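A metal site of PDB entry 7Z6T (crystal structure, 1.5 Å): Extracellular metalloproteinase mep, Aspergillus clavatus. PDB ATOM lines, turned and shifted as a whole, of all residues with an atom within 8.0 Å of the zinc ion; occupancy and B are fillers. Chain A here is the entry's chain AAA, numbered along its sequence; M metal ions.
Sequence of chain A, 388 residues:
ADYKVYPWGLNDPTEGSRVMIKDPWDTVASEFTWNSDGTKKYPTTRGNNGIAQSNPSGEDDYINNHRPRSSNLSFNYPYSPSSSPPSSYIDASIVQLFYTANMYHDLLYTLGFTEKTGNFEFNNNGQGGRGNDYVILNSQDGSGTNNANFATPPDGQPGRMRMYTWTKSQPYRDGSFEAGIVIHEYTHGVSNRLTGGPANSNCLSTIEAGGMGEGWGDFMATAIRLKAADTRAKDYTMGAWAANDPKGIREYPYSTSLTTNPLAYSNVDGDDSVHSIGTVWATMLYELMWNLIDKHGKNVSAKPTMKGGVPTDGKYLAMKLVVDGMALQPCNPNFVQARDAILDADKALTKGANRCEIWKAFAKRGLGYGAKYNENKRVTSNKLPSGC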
ATOM      1  N   ASN A 147      -7.126  22.249 -27.188  1.00  0.00           N
ATOM      2  CA  ASN A 147      -6.094  21.432 -26.554  1.00  0.00           C
ATOM      3  C   ASN A 147      -6.717  20.791 -25.323  1.00  0.00           C
ATOM      4  O   ASN A 147      -7.935  20.806 -25.132  1.00  0.00           O
ATOM      5  CB  ASN A 147      -4.925  22.318 -26.152  1.00  0.00           C
ATOM      6  CG  ASN A 147      -3.577  21.658 -26.352  1.00  0.00           C
ATOM      7  OD1 ASN A 147      -3.438  20.445 -26.158  1.00  0.00           O
ATOM      8  ND2 ASN A 147      -2.584  22.449 -26.737  1.00  0.00           N
ATOM      9  N   ALA A 148      -5.841  20.186 -24.525  1.00  0.00           N
ATOM     10  CA  ALA A 148      -6.161  19.677 -23.199  1.00  0.00           C
ATOM     11  C   ALA A 148      -4.835  19.543 -22.452  1.00  0.00           C
ATOM     12  O   ALA A 148      -3.767  19.624 -23.066  1.00  0.00           O
ATOM     13  CB  ALA A 148      -6.923  18.352 -23.247  1.00  0.00           C
ATOM     14  N   ASN A 149      -4.885  19.333 -21.144  1.00  0.00           N
ATOM     15  CA  ASN A 149      -3.633  19.042 -20.458  1.00  0.00           C
ATOM     16  C   ASN A 149      -3.902  18.316 -19.139  1.00  0.00           C
ATOM     17  O   ASN A 149      -5.033  18.225 -18.655  1.00  0.00           O
ATOM     18  CB  ASN A 149      -2.782  20.295 -20.255  1.00  0.00           C
ATOM     19  CG  ASN A 149      -3.584  21.414 -19.626  1.00  0.00           C
ATOM     20  OD1 ASN A 149      -4.009  21.288 -18.487  1.00  0.00           O
ATOM     21  ND2 ASN A 149      -3.809  22.470 -20.389  1.00  0.00           N
ATOM     22  N   PHE A 150      -2.809  17.760 -18.639  1.00  0.00           N
ATOM     23  CA  PHE A 150      -2.808  16.929 -17.443  1.00  0.00           C
ATOM     24  C   PHE A 150      -1.584  17.301 -16.630  1.00  0.00           C
ATOM     25  O   PHE A 150      -0.507  17.448 -17.193  1.00  0.00           O
ATOM     26  CB  PHE A 150      -2.784  15.437 -17.794  1.00  0.00           C
ATOM     27  CG  PHE A 150      -3.237  14.582 -16.638  1.00  0.00           C
ATOM     28  CD1 PHE A 150      -2.323  14.121 -15.677  1.00  0.00           C
ATOM     29  CD2 PHE A 150      -4.573  14.229 -16.529  1.00  0.00           C
ATOM     30  CE1 PHE A 150      -2.760  13.391 -14.572  1.00  0.00           C
ATOM     31  CE2 PHE A 150      -4.980  13.441 -15.476  1.00  0.00           C
ATOM     32  CZ  PHE A 150      -4.089  12.996 -14.511  1.00  0.00           C
ATOM     33  N   ILE A 181      -9.086  11.982 -26.334  1.00  0.00           N
ATOM     34  CA  ILE A 181      -8.295  13.063 -25.729  1.00  0.00           C
ATOM     35  C   ILE A 181      -8.254  12.887 -24.217  1.00  0.00           C
ATOM     36  O   ILE A 181      -7.207  13.032 -23.593  1.00  0.00           O
ATOM     37  CB  ILE A 181      -8.837  14.449 -26.157  1.00  0.00           C
ATOM     38  CG1 ILE A 181      -8.592  14.622 -27.644  1.00  0.00           C
ATOM     39  CG2 ILE A 181      -8.180  15.566 -25.356  1.00  0.00           C
ATOM     40  CD1 ILE A 181      -9.305  15.869 -28.166  1.00  0.00           C
ATOM     41  N   HIS A 184      -5.846  10.084 -23.590  1.00  0.00           N
ATOM     42  CA  HIS A 184      -4.512  10.603 -23.764  1.00  0.00           C
ATOM     43  C   HIS A 184      -4.036  11.333 -22.517  1.00  0.00           C
ATOM     44  O   HIS A 184      -2.922  11.101 -22.027  1.00  0.00           O
ATOM     45  CB  HIS A 184      -4.394  11.496 -25.017  1.00  0.00           C
ATOM     46  CG  HIS A 184      -3.096  12.220 -25.105  1.00  0.00           C
ATOM     47  ND1 HIS A 184      -2.125  11.898 -26.062  1.00  0.00           N
ATOM     48  CD2 HIS A 184      -2.654  13.275 -24.413  1.00  0.00           C
ATOM     49  CE1 HIS A 184      -1.093  12.723 -25.875  1.00  0.00           C
ATOM     50  NE2 HIS A 184      -1.411  13.586 -24.858  1.00  0.00           N
ATOM     51  N   GLU A 185      -4.832  12.285 -22.058  1.00  0.00           N
ATOM     52  CA  GLU A 185      -4.381  13.081 -20.921  1.00  0.00           C
ATOM     53  C   GLU A 185      -4.224  12.246 -19.654  1.00  0.00           C
ATOM     54  O   GLU A 185      -3.214  12.383 -18.957  1.00  0.00           O
ATOM     55  CB  GLU A 185      -5.346  14.210 -20.648  1.00  0.00           C
ATOM     56  CG  GLU A 185      -5.355  15.196 -21.798  1.00  0.00           C
ATOM     57  CD  GLU A 185      -4.009  15.794 -22.122  1.00  0.00           C
ATOM     58  OE1 GLU A 185      -3.116  15.754 -21.295  1.00  0.00           O
ATOM     59  OE2 GLU A 185      -3.876  16.297 -23.246  1.00  0.00           O
ATOM     60  N   TYR A 186      -5.230  11.405 -19.357  1.00  0.00           N
ATOM     61  CA  TYR A 186      -5.133  10.550 -18.160  1.00  0.00           C
ATOM     62  C   TYR A 186      -3.873   9.674 -18.207  1.00  0.00           C
ATOM     63  O   TYR A 186      -3.231   9.371 -17.195  1.00  0.00           O
ATOM     64  CB  TYR A 186      -6.408   9.709 -18.021  1.00  0.00           C
ATOM     65  CG  TYR A 186      -6.644   9.086 -16.667  1.00  0.00           C
ATOM     66  CD1 TYR A 186      -5.885   8.021 -16.199  1.00  0.00           C
ATOM     67  CD2 TYR A 186      -7.733   9.468 -15.887  1.00  0.00           C
ATOM     68  CE1 TYR A 186      -6.122   7.437 -14.951  1.00  0.00           C
ATOM     69  CE2 TYR A 186      -7.973   8.905 -14.645  1.00  0.00           C
ATOM     70  CZ  TYR A 186      -7.180   7.876 -14.174  1.00  0.00           C
ATOM     71  OH  TYR A 186      -7.421   7.258 -12.971  1.00  0.00           O
ATOM     72  N   THR A 187      -3.497   9.237 -19.423  1.00  0.00           N
ATOM     73  CA  THR A 187      -2.341   8.363 -19.535  1.00  0.00           C
ATOM     74  C   THR A 187      -1.064   9.108 -19.101  1.00  0.00           C
ATOM     75  O   THR A 187      -0.126   8.449 -18.649  1.00  0.00           O
ATOM     76  CB  THR A 187      -2.189   7.841 -20.975  1.00  0.00           C
ATOM     77  OG1 THR A 187      -3.411   7.192 -21.366  1.00  0.00           O
ATOM     78  CG2 THR A 187      -1.053   6.855 -21.114  1.00  0.00           C
ATOM     79  N   HIS A 188      -1.020  10.451 -19.194  1.00  0.00           N
ATOM     80  CA  HIS A 188       0.143  11.161 -18.678  1.00  0.00           C
ATOM     81  C   HIS A 188       0.302  10.895 -17.177  1.00  0.00           C
ATOM     82  O   HIS A 188       1.431  10.856 -16.658  1.00  0.00           O
ATOM     83  CB  HIS A 188       0.008  12.679 -18.905  1.00  0.00           C
ATOM     84  CG  HIS A 188       0.361  13.111 -20.285  1.00  0.00           C
ATOM     85  ND1 HIS A 188       1.631  12.832 -20.806  1.00  0.00           N
ATOM     86  CD2 HIS A 188      -0.349  13.791 -21.223  1.00  0.00           C
ATOM     87  CE1 HIS A 188       1.687  13.342 -22.056  1.00  0.00           C
ATOM     88  NE2 HIS A 188       0.484  13.922 -22.323  1.00  0.00           N
ATOM     89  N   GLY A 210       9.911  12.504 -22.845  1.00  0.00           N
ATOM     90  CA  GLY A 210       8.692  13.296 -22.987  1.00  0.00           C
ATOM     91  C   GLY A 210       7.901  12.944 -24.247  1.00  0.00           C
ATOM     92  O   GLY A 210       6.659  12.947 -24.259  1.00  0.00           O
ATOM     93  N   GLY A 211       8.656  12.622 -25.313  1.00  0.00           N
ATOM     94  CA  GLY A 211       8.057  12.115 -26.547  1.00  0.00           C
ATOM     95  C   GLY A 211       7.263  10.831 -26.323  1.00  0.00           C
ATOM     96  O   GLY A 211       6.094  10.771 -26.735  1.00  0.00           O
ATOM     97  N   GLY A 213       6.120  10.020 -23.611  1.00  0.00           N
ATOM     98  CA  GLY A 213       4.997  10.482 -22.796  1.00  0.00           C
ATOM     99  C   GLY A 213       3.756  10.800 -23.630  1.00  0.00           C
ATOM    100  O   GLY A 213       2.653  10.437 -23.272  1.00  0.00           O
ATOM    101  N   GLU A 214       3.957  11.483 -24.769  1.00  0.00           N
ATOM    102  CA  GLU A 214       2.830  11.789 -25.652  1.00  0.00           C
ATOM    103  C   GLU A 214       2.353  10.527 -26.375  1.00  0.00           C
ATOM    104  O   GLU A 214       1.139  10.315 -26.484  1.00  0.00           O
ATOM    105  CB  GLU A 214       3.234  12.869 -26.669  1.00  0.00           C
ATOM    106  CG  GLU A 214       3.694  14.158 -26.002  1.00  0.00           C
ATOM    107  CD  GLU A 214       2.638  14.761 -25.097  1.00  0.00           C
ATOM    108  OE1 GLU A 214       1.428  14.552 -25.398  1.00  0.00           O
ATOM    109  OE2 GLU A 214       3.025  15.447 -24.106  1.00  0.00           O
ATOM    110  N   GLY A 215       3.314   9.680 -26.796  1.00  0.00           N
ATOM    111  CA  GLY A 215       2.911   8.510 -27.559  1.00  0.00           C
ATOM    112  C   GLY A 215       2.077   7.521 -26.748  1.00  0.00           C
ATOM    113  O   GLY A 215       1.207   6.870 -27.300  1.00  0.00           O
ATOM    114  N   TRP A 216       2.421   7.326 -25.469  1.00  0.00           N
ATOM    115  CA  TRP A 216       1.680   6.324 -24.726  1.00  0.00           C
ATOM    116  C   TRP A 216       0.200   6.680 -24.699  1.00  0.00           C
ATOM    117  O   TRP A 216      -0.658   5.808 -24.791  1.00  0.00           O
ATOM    118  CB  TRP A 216       2.220   6.188 -23.287  1.00  0.00           C
ATOM    119  CG  TRP A 216       3.468   5.344 -23.176  1.00  0.00           C
ATOM    120  CD1 TRP A 216       3.649   4.040 -23.556  1.00  0.00           C
ATOM    121  CD2 TRP A 216       4.680   5.753 -22.528  1.00  0.00           C
ATOM    122  NE1 TRP A 216       4.906   3.620 -23.195  1.00  0.00           N
ATOM    123  CE2 TRP A 216       5.581   4.665 -22.620  1.00  0.00           C
ATOM    124  CE3 TRP A 216       5.105   6.945 -21.936  1.00  0.00           C
ATOM    125  CZ2 TRP A 216       6.866   4.725 -22.093  1.00  0.00           C
ATOM    126  CZ3 TRP A 216       6.371   6.991 -21.400  1.00  0.00           C
ATOM    127  CH2 TRP A 216       7.258   5.925 -21.517  1.00  0.00           C
ATOM    128  N   GLY A 217      -0.116   7.967 -24.548  1.00  0.00           N
ATOM    129  CA  GLY A 217      -1.507   8.396 -24.494  1.00  0.00           C
ATOM    130  C   GLY A 217      -2.234   8.235 -25.839  1.00  0.00           C
ATOM    131  O   GLY A 217      -3.397   7.812 -25.862  1.00  0.00           O
ATOM    132  N   ASP A 218      -1.546   8.486 -26.952  1.00  0.00           N
ATOM    133  CA  ASP A 218      -2.130   8.273 -28.262  1.00  0.00           C
ATOM    134  C   ASP A 218      -2.358   6.786 -28.487  1.00  0.00           C
ATOM    135  O   ASP A 218      -3.403   6.373 -28.992  1.00  0.00           O
ATOM    136  CB  ASP A 218      -1.190   8.820 -29.332  1.00  0.00           C
ATOM    137  CG  ASP A 218      -1.282  10.325 -29.553  1.00  0.00           C
ATOM    138  OD1 ASP A 218      -1.780  11.046 -28.691  1.00  0.00           O
ATOM    139  OD2 ASP A 218      -0.790  10.762 -30.636  1.00  0.00           O
ATOM    140  N   ARG A 250      -1.825  14.719 -35.638  1.00  0.00           N
ATOM    141  CA  ARG A 250      -0.447  14.292 -35.782  1.00  0.00           C
ATOM    142  C   ARG A 250      -0.087  14.283 -37.284  1.00  0.00           C
ATOM    143  O   ARG A 250      -0.957  14.467 -38.149  1.00  0.00           O
ATOM    144  CB  ARG A 250      -0.235  12.901 -35.184  1.00  0.00           C
ATOM    145  CG  ARG A 250      -0.758  12.740 -33.761  1.00  0.00           C
ATOM    146  CD  ARG A 250      -0.071  13.666 -32.779  1.00  0.00           C
ATOM    147  NE  ARG A 250      -0.592  13.366 -31.439  1.00  0.00           N
ATOM    148  CZ  ARG A 250      -0.748  14.233 -30.461  1.00  0.00           C
ATOM    149  NH1 ARG A 250      -0.484  15.532 -30.613  1.00  0.00           N
ATOM    150  NH2 ARG A 250      -1.197  13.800 -29.298  1.00  0.00           N
ATOM    151  N   VAL A 274       7.796  17.086 -28.560  1.00  0.00           N
ATOM    152  CA  VAL A 274       7.436  15.821 -27.920  1.00  0.00           C
ATOM    153  C   VAL A 274       6.234  15.185 -28.615  1.00  0.00           C
ATOM    154  O   VAL A 274       6.138  13.950 -28.603  1.00  0.00           O
ATOM    155  CB  VAL A 274       7.164  15.959 -26.413  1.00  0.00           C
ATOM    156  CG1 VAL A 274       8.448  16.277 -25.642  1.00  0.00           C
ATOM    157  CG2 VAL A 274       6.065  16.987 -26.117  1.00  0.00           C
ATOM    158  N   HIS A 275       5.316  15.994 -29.206  1.00  0.00           N
ATOM    159  CA  HIS A 275       4.160  15.390 -29.857  1.00  0.00           C
ATOM    160  C   HIS A 275       4.560  14.649 -31.133  1.00  0.00           C
ATOM    161  O   HIS A 275       3.974  13.602 -31.420  1.00  0.00           O
ATOM    162  CB  HIS A 275       3.084  16.433 -30.169  1.00  0.00           C
ATOM    163  CG  HIS A 275       2.607  17.038 -28.900  1.00  0.00           C
ATOM    164  ND1 HIS A 275       3.147  18.199 -28.420  1.00  0.00           N
ATOM    165  CD2 HIS A 275       1.715  16.599 -27.988  1.00  0.00           C
ATOM    166  CE1 HIS A 275       2.597  18.474 -27.230  1.00  0.00           C
ATOM    167  NE2 HIS A 275       1.690  17.534 -26.965  1.00  0.00           N
HETATM  168 ZN    ZN M   1      -0.025  14.782 -24.054  1.00  0.00          ZN
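The side-chain carboxylate (OE1) of Glu 214 lies close to a ring nitrogen (NE2) of His 275 (3.4 Å). OD1 of Asp 218 is in hydrogen-bond range of ND1 of His 184, 2.8 Å away.
Of the 21 residues printed, 3 come within 4 Å of the zinc ion.
OE1 of Glu 214 is bound to the zinc ion (2.0 Å). The zinc ion is bound by NE2 of His 188. The zinc ion is bound by NE2 of His 184 (2.0 Å).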
